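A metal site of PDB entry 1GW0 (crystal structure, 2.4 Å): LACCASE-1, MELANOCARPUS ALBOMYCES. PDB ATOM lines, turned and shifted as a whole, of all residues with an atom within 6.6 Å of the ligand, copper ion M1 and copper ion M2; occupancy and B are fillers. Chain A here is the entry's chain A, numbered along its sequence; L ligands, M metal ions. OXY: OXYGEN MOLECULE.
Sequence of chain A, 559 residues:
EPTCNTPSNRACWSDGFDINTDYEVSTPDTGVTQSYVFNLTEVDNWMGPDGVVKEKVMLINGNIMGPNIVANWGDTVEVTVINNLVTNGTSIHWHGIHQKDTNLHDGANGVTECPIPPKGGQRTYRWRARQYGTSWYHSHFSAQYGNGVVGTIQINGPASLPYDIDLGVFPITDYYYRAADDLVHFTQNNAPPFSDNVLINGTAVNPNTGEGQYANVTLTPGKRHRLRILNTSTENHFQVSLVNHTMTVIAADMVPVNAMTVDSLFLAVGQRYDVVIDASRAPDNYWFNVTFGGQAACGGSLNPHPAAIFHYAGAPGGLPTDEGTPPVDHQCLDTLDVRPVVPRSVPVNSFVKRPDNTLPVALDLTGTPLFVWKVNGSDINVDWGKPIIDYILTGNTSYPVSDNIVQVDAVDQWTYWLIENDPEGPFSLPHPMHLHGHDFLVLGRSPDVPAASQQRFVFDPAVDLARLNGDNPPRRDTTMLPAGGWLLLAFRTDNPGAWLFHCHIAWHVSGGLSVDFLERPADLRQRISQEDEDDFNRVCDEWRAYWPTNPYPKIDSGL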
ATOM      1  N   HIS A  93     -28.781  27.055  25.228  1.00  0.00           N
ATOM      2  CA  HIS A  93     -27.687  28.007  25.230  1.00  0.00           C
ATOM      3  C   HIS A  93     -28.096  29.168  24.334  1.00  0.00           C
ATOM      4  O   HIS A  93     -28.723  28.969  23.278  1.00  0.00           O
ATOM      5  CB  HIS A  93     -26.411  27.337  24.712  1.00  0.00           C
ATOM      6  CG  HIS A  93     -25.353  28.309  24.284  1.00  0.00           C
ATOM      7  ND1 HIS A  93     -24.780  29.217  25.157  1.00  0.00           N
ATOM      8  CD2 HIS A  93     -24.792  28.543  23.074  1.00  0.00           C
ATOM      9  CE1 HIS A  93     -23.914  29.963  24.495  1.00  0.00           C
ATOM     10  NE2 HIS A  93     -23.905  29.575  23.236  1.00  0.00           N
ATOM     11  N   TRP A  94     -27.761  30.380  24.766  1.00  0.00           N
ATOM     12  CA  TRP A  94     -28.109  31.590  24.043  1.00  0.00           C
ATOM     13  C   TRP A  94     -26.882  32.094  23.293  1.00  0.00           C
ATOM     14  O   TRP A  94     -26.137  32.952  23.776  1.00  0.00           O
ATOM     15  CB  TRP A  94     -28.656  32.640  25.019  1.00  0.00           C
ATOM     16  CG  TRP A  94     -29.553  32.024  26.064  1.00  0.00           C
ATOM     17  CD1 TRP A  94     -29.169  31.514  27.280  1.00  0.00           C
ATOM     18  CD2 TRP A  94     -30.946  31.713  25.920  1.00  0.00           C
ATOM     19  NE1 TRP A  94     -30.233  30.884  27.881  1.00  0.00           N
ATOM     20  CE2 TRP A  94     -31.332  31.004  27.078  1.00  0.00           C
ATOM     21  CE3 TRP A  94     -31.899  31.964  24.927  1.00  0.00           C
ATOM     22  CZ2 TRP A  94     -32.634  30.525  27.258  1.00  0.00           C
ATOM     23  CZ3 TRP A  94     -33.193  31.491  25.108  1.00  0.00           C
ATOM     24  CH2 TRP A  94     -33.550  30.774  26.265  1.00  0.00           C
ATOM     25  N   HIS A  95     -26.683  31.528  22.110  1.00  0.00           N
ATOM     26  CA  HIS A  95     -25.564  31.811  21.221  1.00  0.00           C
ATOM     27  C   HIS A  95     -25.434  33.287  20.837  1.00  0.00           C
ATOM     28  O   HIS A  95     -26.221  33.795  20.041  1.00  0.00           O
ATOM     29  CB  HIS A  95     -25.725  30.960  19.958  1.00  0.00           C
ATOM     30  CG  HIS A  95     -24.514  30.945  19.087  1.00  0.00           C
ATOM     31  ND1 HIS A  95     -23.759  29.799  18.884  1.00  0.00           N
ATOM     32  CD2 HIS A  95     -23.915  31.914  18.362  1.00  0.00           C
ATOM     33  CE1 HIS A  95     -22.762  30.078  18.072  1.00  0.00           C
ATOM     34  NE2 HIS A  95     -22.831  31.356  17.733  1.00  0.00           N
ATOM     35  N   GLY A  96     -24.423  33.960  21.383  1.00  0.00           N
ATOM     36  CA  GLY A  96     -24.225  35.358  21.069  1.00  0.00           C
ATOM     37  C   GLY A  96     -24.414  36.241  22.288  1.00  0.00           C
ATOM     38  O   GLY A  96     -23.936  37.374  22.329  1.00  0.00           O
ATOM     39  N   ASP A 106     -25.881  30.423  31.057  1.00  0.00           N
ATOM     40  CA  ASP A 106     -25.322  30.208  29.722  1.00  0.00           C
ATOM     41  C   ASP A 106     -25.904  28.992  29.014  1.00  0.00           C
ATOM     42  O   ASP A 106     -25.946  28.943  27.780  1.00  0.00           O
ATOM     43  CB  ASP A 106     -23.787  30.078  29.796  1.00  0.00           C
ATOM     44  CG  ASP A 106     -23.135  30.077  28.428  1.00  0.00           C
ATOM     45  OD1 ASP A 106     -23.407  31.007  27.639  1.00  0.00           O
ATOM     46  OD2 ASP A 106     -22.341  29.160  28.151  1.00  0.00           O
ATOM     47  N   ALA A 108     -24.809  25.711  29.258  1.00  0.00           N
ATOM     48  CA  ALA A 108     -23.786  24.751  28.849  1.00  0.00           C
ATOM     49  C   ALA A 108     -23.823  23.556  29.800  1.00  0.00           C
ATOM     50  O   ALA A 108     -23.082  23.530  30.774  1.00  0.00           O
ATOM     51  CB  ALA A 108     -22.424  25.424  28.898  1.00  0.00           C
ATOM     52  N   TRP A 136     -29.128  33.692  18.154  1.00  0.00           N
ATOM     53  CA  TRP A 136     -30.014  32.542  18.151  1.00  0.00           C
ATOM     54  C   TRP A 136     -29.773  31.661  19.366  1.00  0.00           C
ATOM     55  O   TRP A 136     -28.812  31.879  20.107  1.00  0.00           O
ATOM     56  CB  TRP A 136     -29.823  31.740  16.858  1.00  0.00           C
ATOM     57  CG  TRP A 136     -28.422  31.167  16.655  1.00  0.00           C
ATOM     58  CD1 TRP A 136     -27.236  31.859  16.676  1.00  0.00           C
ATOM     59  CD2 TRP A 136     -28.078  29.797  16.385  1.00  0.00           C
ATOM     60  NE1 TRP A 136     -26.183  30.997  16.429  1.00  0.00           N
ATOM     61  CE2 TRP A 136     -26.674  29.736  16.248  1.00  0.00           C
ATOM     62  CE3 TRP A 136     -28.836  28.615  16.242  1.00  0.00           C
ATOM     63  CZ2 TRP A 136     -26.010  28.535  15.983  1.00  0.00           C
ATOM     64  CZ3 TRP A 136     -28.166  27.425  15.965  1.00  0.00           C
ATOM     65  CH2 TRP A 136     -26.760  27.395  15.841  1.00  0.00           C
ATOM     66  N   TYR A 137     -30.642  30.679  19.589  1.00  0.00           N
ATOM     67  CA  TYR A 137     -30.477  29.797  20.731  1.00  0.00           C
ATOM     68  C   TYR A 137     -30.675  28.372  20.274  1.00  0.00           C
ATOM     69  O   TYR A 137     -31.332  28.121  19.257  1.00  0.00           O
ATOM     70  CB  TYR A 137     -31.475  30.134  21.858  1.00  0.00           C
ATOM     71  CG  TYR A 137     -32.930  30.127  21.435  1.00  0.00           C
ATOM     72  CD1 TYR A 137     -33.542  31.274  20.939  1.00  0.00           C
ATOM     73  CD2 TYR A 137     -33.672  28.950  21.487  1.00  0.00           C
ATOM     74  CE1 TYR A 137     -34.878  31.252  20.487  1.00  0.00           C
ATOM     75  CE2 TYR A 137     -34.996  28.906  21.054  1.00  0.00           C
ATOM     76  CZ  TYR A 137     -35.589  30.061  20.550  1.00  0.00           C
ATOM     77  OH  TYR A 137     -36.891  29.985  20.099  1.00  0.00           O
ATOM     78  N   HIS A 138     -30.103  27.443  21.022  1.00  0.00           N
ATOM     79  CA  HIS A 138     -30.213  26.032  20.679  1.00  0.00           C
ATOM     80  C   HIS A 138     -29.798  25.162  21.850  1.00  0.00           C
ATOM     81  O   HIS A 138     -29.149  25.623  22.788  1.00  0.00           O
ATOM     82  CB  HIS A 138     -29.330  25.718  19.475  1.00  0.00           C
ATOM     83  CG  HIS A 138     -27.894  26.105  19.652  1.00  0.00           C
ATOM     84  ND1 HIS A 138     -27.031  25.402  20.466  1.00  0.00           N
ATOM     85  CD2 HIS A 138     -27.177  27.140  19.152  1.00  0.00           C
ATOM     86  CE1 HIS A 138     -25.843  25.983  20.453  1.00  0.00           C
ATOM     87  NE2 HIS A 138     -25.898  27.038  19.655  1.00  0.00           N
ATOM     88  N   SER A 139     -30.189  23.893  21.803  1.00  0.00           N
ATOM     89  CA  SER A 139     -29.826  22.954  22.852  1.00  0.00           C
ATOM     90  C   SER A 139     -28.317  22.715  22.789  1.00  0.00           C
ATOM     91  O   SER A 139     -27.681  22.922  21.734  1.00  0.00           O
ATOM     92  CB  SER A 139     -30.561  21.631  22.635  1.00  0.00           C
ATOM     93  OG  SER A 139     -30.163  20.670  23.582  1.00  0.00           O
ATOM     94  N   HIS A 140     -27.733  22.298  23.914  1.00  0.00           N
ATOM     95  CA  HIS A 140     -26.304  22.000  23.975  1.00  0.00           C
ATOM     96  C   HIS A 140     -26.168  20.585  24.539  1.00  0.00           C
ATOM     97  O   HIS A 140     -25.081  20.167  24.917  1.00  0.00           O
ATOM     98  CB  HIS A 140     -25.558  23.007  24.866  1.00  0.00           C
ATOM     99  CG  HIS A 140     -24.281  23.528  24.262  1.00  0.00           C
ATOM    100  ND1 HIS A 140     -23.331  22.703  23.692  1.00  0.00           N
ATOM    101  CD2 HIS A 140     -23.806  24.799  24.138  1.00  0.00           C
ATOM    102  CE1 HIS A 140     -22.333  23.438  23.227  1.00  0.00           C
ATOM    103  NE2 HIS A 140     -22.593  24.714  23.479  1.00  0.00           N
ATOM    104  N   TYR A 145     -30.008  19.734  19.255  1.00  0.00           N
ATOM    105  CA  TYR A 145     -30.585  20.823  18.484  1.00  0.00           C
ATOM    106  C   TYR A 145     -30.706  20.482  17.020  1.00  0.00           C
ATOM    107  O   TYR A 145     -31.276  21.224  16.238  1.00  0.00           O
ATOM    108  CB  TYR A 145     -29.795  22.132  18.708  1.00  0.00           C
ATOM    109  CG  TYR A 145     -28.657  22.469  17.746  1.00  0.00           C
ATOM    110  CD1 TYR A 145     -28.912  22.969  16.470  1.00  0.00           C
ATOM    111  CD2 TYR A 145     -27.337  22.353  18.157  1.00  0.00           C
ATOM    112  CE1 TYR A 145     -27.867  23.363  15.628  1.00  0.00           C
ATOM    113  CE2 TYR A 145     -26.276  22.739  17.332  1.00  0.00           C
ATOM    114  CZ  TYR A 145     -26.549  23.246  16.070  1.00  0.00           C
ATOM    115  OH  TYR A 145     -25.496  23.639  15.274  1.00  0.00           O
ATOM    116  N   GLY A 270     -23.364  28.921  12.705  1.00  0.00           N
ATOM    117  CA  GLY A 270     -23.483  29.816  13.852  1.00  0.00           C
ATOM    118  C   GLY A 270     -23.309  31.317  13.611  1.00  0.00           C
ATOM    119  O   GLY A 270     -23.551  32.101  14.523  1.00  0.00           O
ATOM    120  N   HIS A 434     -16.121  28.700  17.908  1.00  0.00           N
ATOM    121  CA  HIS A 434     -17.030  29.588  18.632  1.00  0.00           C
ATOM    122  C   HIS A 434     -16.719  29.684  20.125  1.00  0.00           C
ATOM    123  O   HIS A 434     -16.404  28.703  20.789  1.00  0.00           O
ATOM    124  CB  HIS A 434     -18.469  29.097  18.418  1.00  0.00           C
ATOM    125  CG  HIS A 434     -19.463  29.696  19.368  1.00  0.00           C
ATOM    126  ND1 HIS A 434     -19.788  31.035  19.363  1.00  0.00           N
ATOM    127  CD2 HIS A 434     -20.178  29.134  20.371  1.00  0.00           C
ATOM    128  CE1 HIS A 434     -20.669  31.268  20.313  1.00  0.00           C
ATOM    129  NE2 HIS A 434     -20.925  30.143  20.944  1.00  0.00           N
ATOM    130  N   HIS A 436     -18.092  31.053  23.972  1.00  0.00           N
ATOM    131  CA  HIS A 436     -19.188  31.487  24.823  1.00  0.00           C
ATOM    132  C   HIS A 436     -18.648  32.636  25.697  1.00  0.00           C
ATOM    133  O   HIS A 436     -17.442  32.720  25.951  1.00  0.00           O
ATOM    134  CB  HIS A 436     -19.653  30.370  25.772  1.00  0.00           C
ATOM    135  CG  HIS A 436     -20.369  29.229  25.106  1.00  0.00           C
ATOM    136  ND1 HIS A 436     -21.189  28.367  25.811  1.00  0.00           N
ATOM    137  CD2 HIS A 436     -20.347  28.767  23.828  1.00  0.00           C
ATOM    138  CE1 HIS A 436     -21.635  27.421  24.991  1.00  0.00           C
ATOM    139  NE2 HIS A 436     -21.140  27.644  23.789  1.00  0.00           N
ATOM    140  N   LEU A 500     -17.165  27.690  27.350  1.00  0.00           N
ATOM    141  CA  LEU A 500     -16.781  26.734  26.329  1.00  0.00           C
ATOM    142  C   LEU A 500     -16.281  27.479  25.094  1.00  0.00           C
ATOM    143  O   LEU A 500     -16.728  28.602  24.775  1.00  0.00           O
ATOM    144  CB  LEU A 500     -17.969  25.851  25.943  1.00  0.00           C
ATOM    145  CG  LEU A 500     -18.383  24.759  26.941  1.00  0.00           C
ATOM    146  CD1 LEU A 500     -19.642  24.096  26.446  1.00  0.00           C
ATOM    147  CD2 LEU A 500     -17.275  23.736  27.115  1.00  0.00           C
ATOM    148  N   PHE A 501     -15.311  26.844  24.414  1.00  0.00           N
ATOM    149  CA  PHE A 501     -14.713  27.340  23.186  1.00  0.00           C
ATOM    150  C   PHE A 501     -14.637  26.058  22.355  1.00  0.00           C
ATOM    151  O   PHE A 501     -13.746  25.223  22.551  1.00  0.00           O
ATOM    152  CB  PHE A 501     -13.324  27.922  23.449  1.00  0.00           C
ATOM    153  CG  PHE A 501     -12.632  28.421  22.211  1.00  0.00           C
ATOM    154  CD1 PHE A 501     -13.238  29.375  21.395  1.00  0.00           C
ATOM    155  CD2 PHE A 501     -11.405  27.919  21.838  1.00  0.00           C
ATOM    156  CE1 PHE A 501     -12.631  29.812  20.217  1.00  0.00           C
ATOM    157  CE2 PHE A 501     -10.771  28.350  20.668  1.00  0.00           C
ATOM    158  CZ  PHE A 501     -11.394  29.294  19.851  1.00  0.00           C
ATOM    159  N   HIS A 502     -15.570  25.894  21.436  1.00  0.00           N
ATOM    160  CA  HIS A 502     -15.636  24.680  20.646  1.00  0.00           C
ATOM    161  C   HIS A 502     -15.894  24.910  19.175  1.00  0.00           C
ATOM    162  O   HIS A 502     -16.100  26.042  18.744  1.00  0.00           O
ATOM    163  CB  HIS A 502     -16.728  23.777  21.229  1.00  0.00           C
ATOM    164  CG  HIS A 502     -18.094  24.394  21.248  1.00  0.00           C
ATOM    165  ND1 HIS A 502     -18.921  24.426  20.143  1.00  0.00           N
ATOM    166  CD2 HIS A 502     -18.786  25.016  22.237  1.00  0.00           C
ATOM    167  CE1 HIS A 502     -20.049  25.022  20.452  1.00  0.00           C
ATOM    168  NE2 HIS A 502     -20.003  25.396  21.718  1.00  0.00           N
ATOM    169  N   HIS A 504     -18.362  24.532  16.130  1.00  0.00           N
ATOM    170  CA  HIS A 504     -19.822  24.426  16.095  1.00  0.00           C
ATOM    171  C   HIS A 504     -20.410  23.358  15.187  1.00  0.00           C
ATOM    172  O   HIS A 504     -21.620  23.286  15.025  1.00  0.00           O
ATOM    173  CB  HIS A 504     -20.453  25.783  15.772  1.00  0.00           C
ATOM    174  CG  HIS A 504     -21.679  26.074  16.586  1.00  0.00           C
ATOM    175  ND1 HIS A 504     -22.847  25.349  16.461  1.00  0.00           N
ATOM    176  CD2 HIS A 504     -21.913  27.007  17.545  1.00  0.00           C
ATOM    177  CE1 HIS A 504     -23.744  25.827  17.309  1.00  0.00           C
ATOM    178  NE2 HIS A 504     -23.210  26.823  17.978  1.00  0.00           N
ATOM    179  N   VAL A 509     -17.851  18.714  17.854  1.00  0.00           N
ATOM    180  CA  VAL A 509     -17.893  19.019  19.286  1.00  0.00           C
ATOM    181  C   VAL A 509     -18.335  17.745  20.006  1.00  0.00           C
ATOM    182  O   VAL A 509     -17.848  17.412  21.084  1.00  0.00           O
ATOM    183  CB  VAL A 509     -18.902  20.158  19.598  1.00  0.00           C
ATOM    184  CG1 VAL A 509     -20.346  19.672  19.402  1.00  0.00           C
ATOM    185  CG2 VAL A 509     -18.680  20.685  21.006  1.00  0.00           C
ATOM    186  N   LEU A 559     -21.566  17.496  24.676  1.00  0.00           N
ATOM    187  CA  LEU A 559     -21.683  18.870  24.192  1.00  0.00           C
ATOM    188  C   LEU A 559     -22.187  18.980  22.755  1.00  0.00           C
ATOM    189  O   LEU A 559     -22.651  20.082  22.383  1.00  0.00           O
ATOM    190  CB  LEU A 559     -20.317  19.585  24.306  1.00  0.00           C
ATOM    191  CG  LEU A 559     -19.755  19.725  25.724  1.00  0.00           C
ATOM    192  CD1 LEU A 559     -18.495  20.605  25.703  1.00  0.00           C
ATOM    193  CD2 LEU A 559     -20.816  20.340  26.632  1.00  0.00           C
ATOM    194  OXT LEU A 559     -22.114  17.971  22.020  1.00  0.00           O
HETATM  195  O1  OXY L   1     -22.762  27.667  20.937  1.00  0.00           O
HETATM  196  O2  OXY L   1     -23.025  26.488  20.803  1.00  0.00           O
HETATM  197 CU    CU M   1     -21.557  26.150  22.654  1.00  0.00          CU
HETATM  198 CU    CU M   2     -24.341  27.998  19.048  1.00  0.00          CU
HETATM  199 CU    CU M   3     -22.399  29.946  22.156  1.00  0.00          CU
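Copper ion M2 is bound by ND1 of His 95 (1.9 Å), NE2 of His 138 (1.9 Å), NE2 of His 504 (2.0 Å) and O1 of the ligand (2.5 Å).
Copper ion M1 is bound by a ring nitrogen (NE2) of His 436 (1.9 Å).
Copper ion M1 is bound by NE2 of His 140.
Copper ion M1 is bound by a ring nitrogen (NE2) of His 502 (2.0 Å).
An oxygen (O2) of the ligand is bound to copper ion M1 (2.4 Å).
Copper ion M1 has four donor atoms within binding distance.
Trp 136 touches copper ion M2 (CZ2 to CU, 3.5 Å).
Four residues have an atom within 4 Å of copper ion M2: His 95, Trp 136, His 138 and His 504.
Along chain A the residues within 4 Å of copper ion M2 span positions 95 to 504.
The nearest printed residue that does not touch copper ion M2 is His 93 (4.1 Å).
N of His 95 is in hydrogen-bond range of O of Trp 136, at 2.9 Å.
NE2 of His 95 is in hydrogen-bond range of O of Gly 270 (3.4 Å).
The backbone NH (N) of His 436 is in hydrogen-bond range of the backbone carbonyl oxygen (O) of Leu 500 (2.9 Å).
A ring nitrogen (ND1) of His 436 is in hydrogen-bond range of the side-chain carboxylate (OD2) of Asp 106.
N of His 93 is in hydrogen-bond range of O of His 138 (2.9 Å).
A ring nitrogen (ND1) of His 504 sits at hydrogen-bond distance from the side-chain hydroxyl of Tyr 145, at 3.4 Å.
The backbone carbonyl oxygen (O) of His 502 lies within hydrogen-bond range of the backbone NH (N) of His 434 (2.8 Å).
The indole nitrogen of Trp 136 is in hydrogen-bond range of the backbone carbonyl oxygen of Gly 270.
NE2 of His 93 sits close to O1 of the ligand.
An oxygen (O1) of the ligand sits close to a ring nitrogen (NE2) of His 434 (3.1 Å).
Hydrophobic or aromatic side chains within 4 Å of the ligand: His 93, His 95, His 138, His 140, His 434, His 436, His 502 and His 504.
The nearest printed residue that does not touch the ligand is Ser 139 (5.9 Å).
Within 4 Å of copper ion M1: His 140, His 436 and His 502.
The nearest printed residue that does not touch copper ion M1 is His 434 (4.002 Å).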
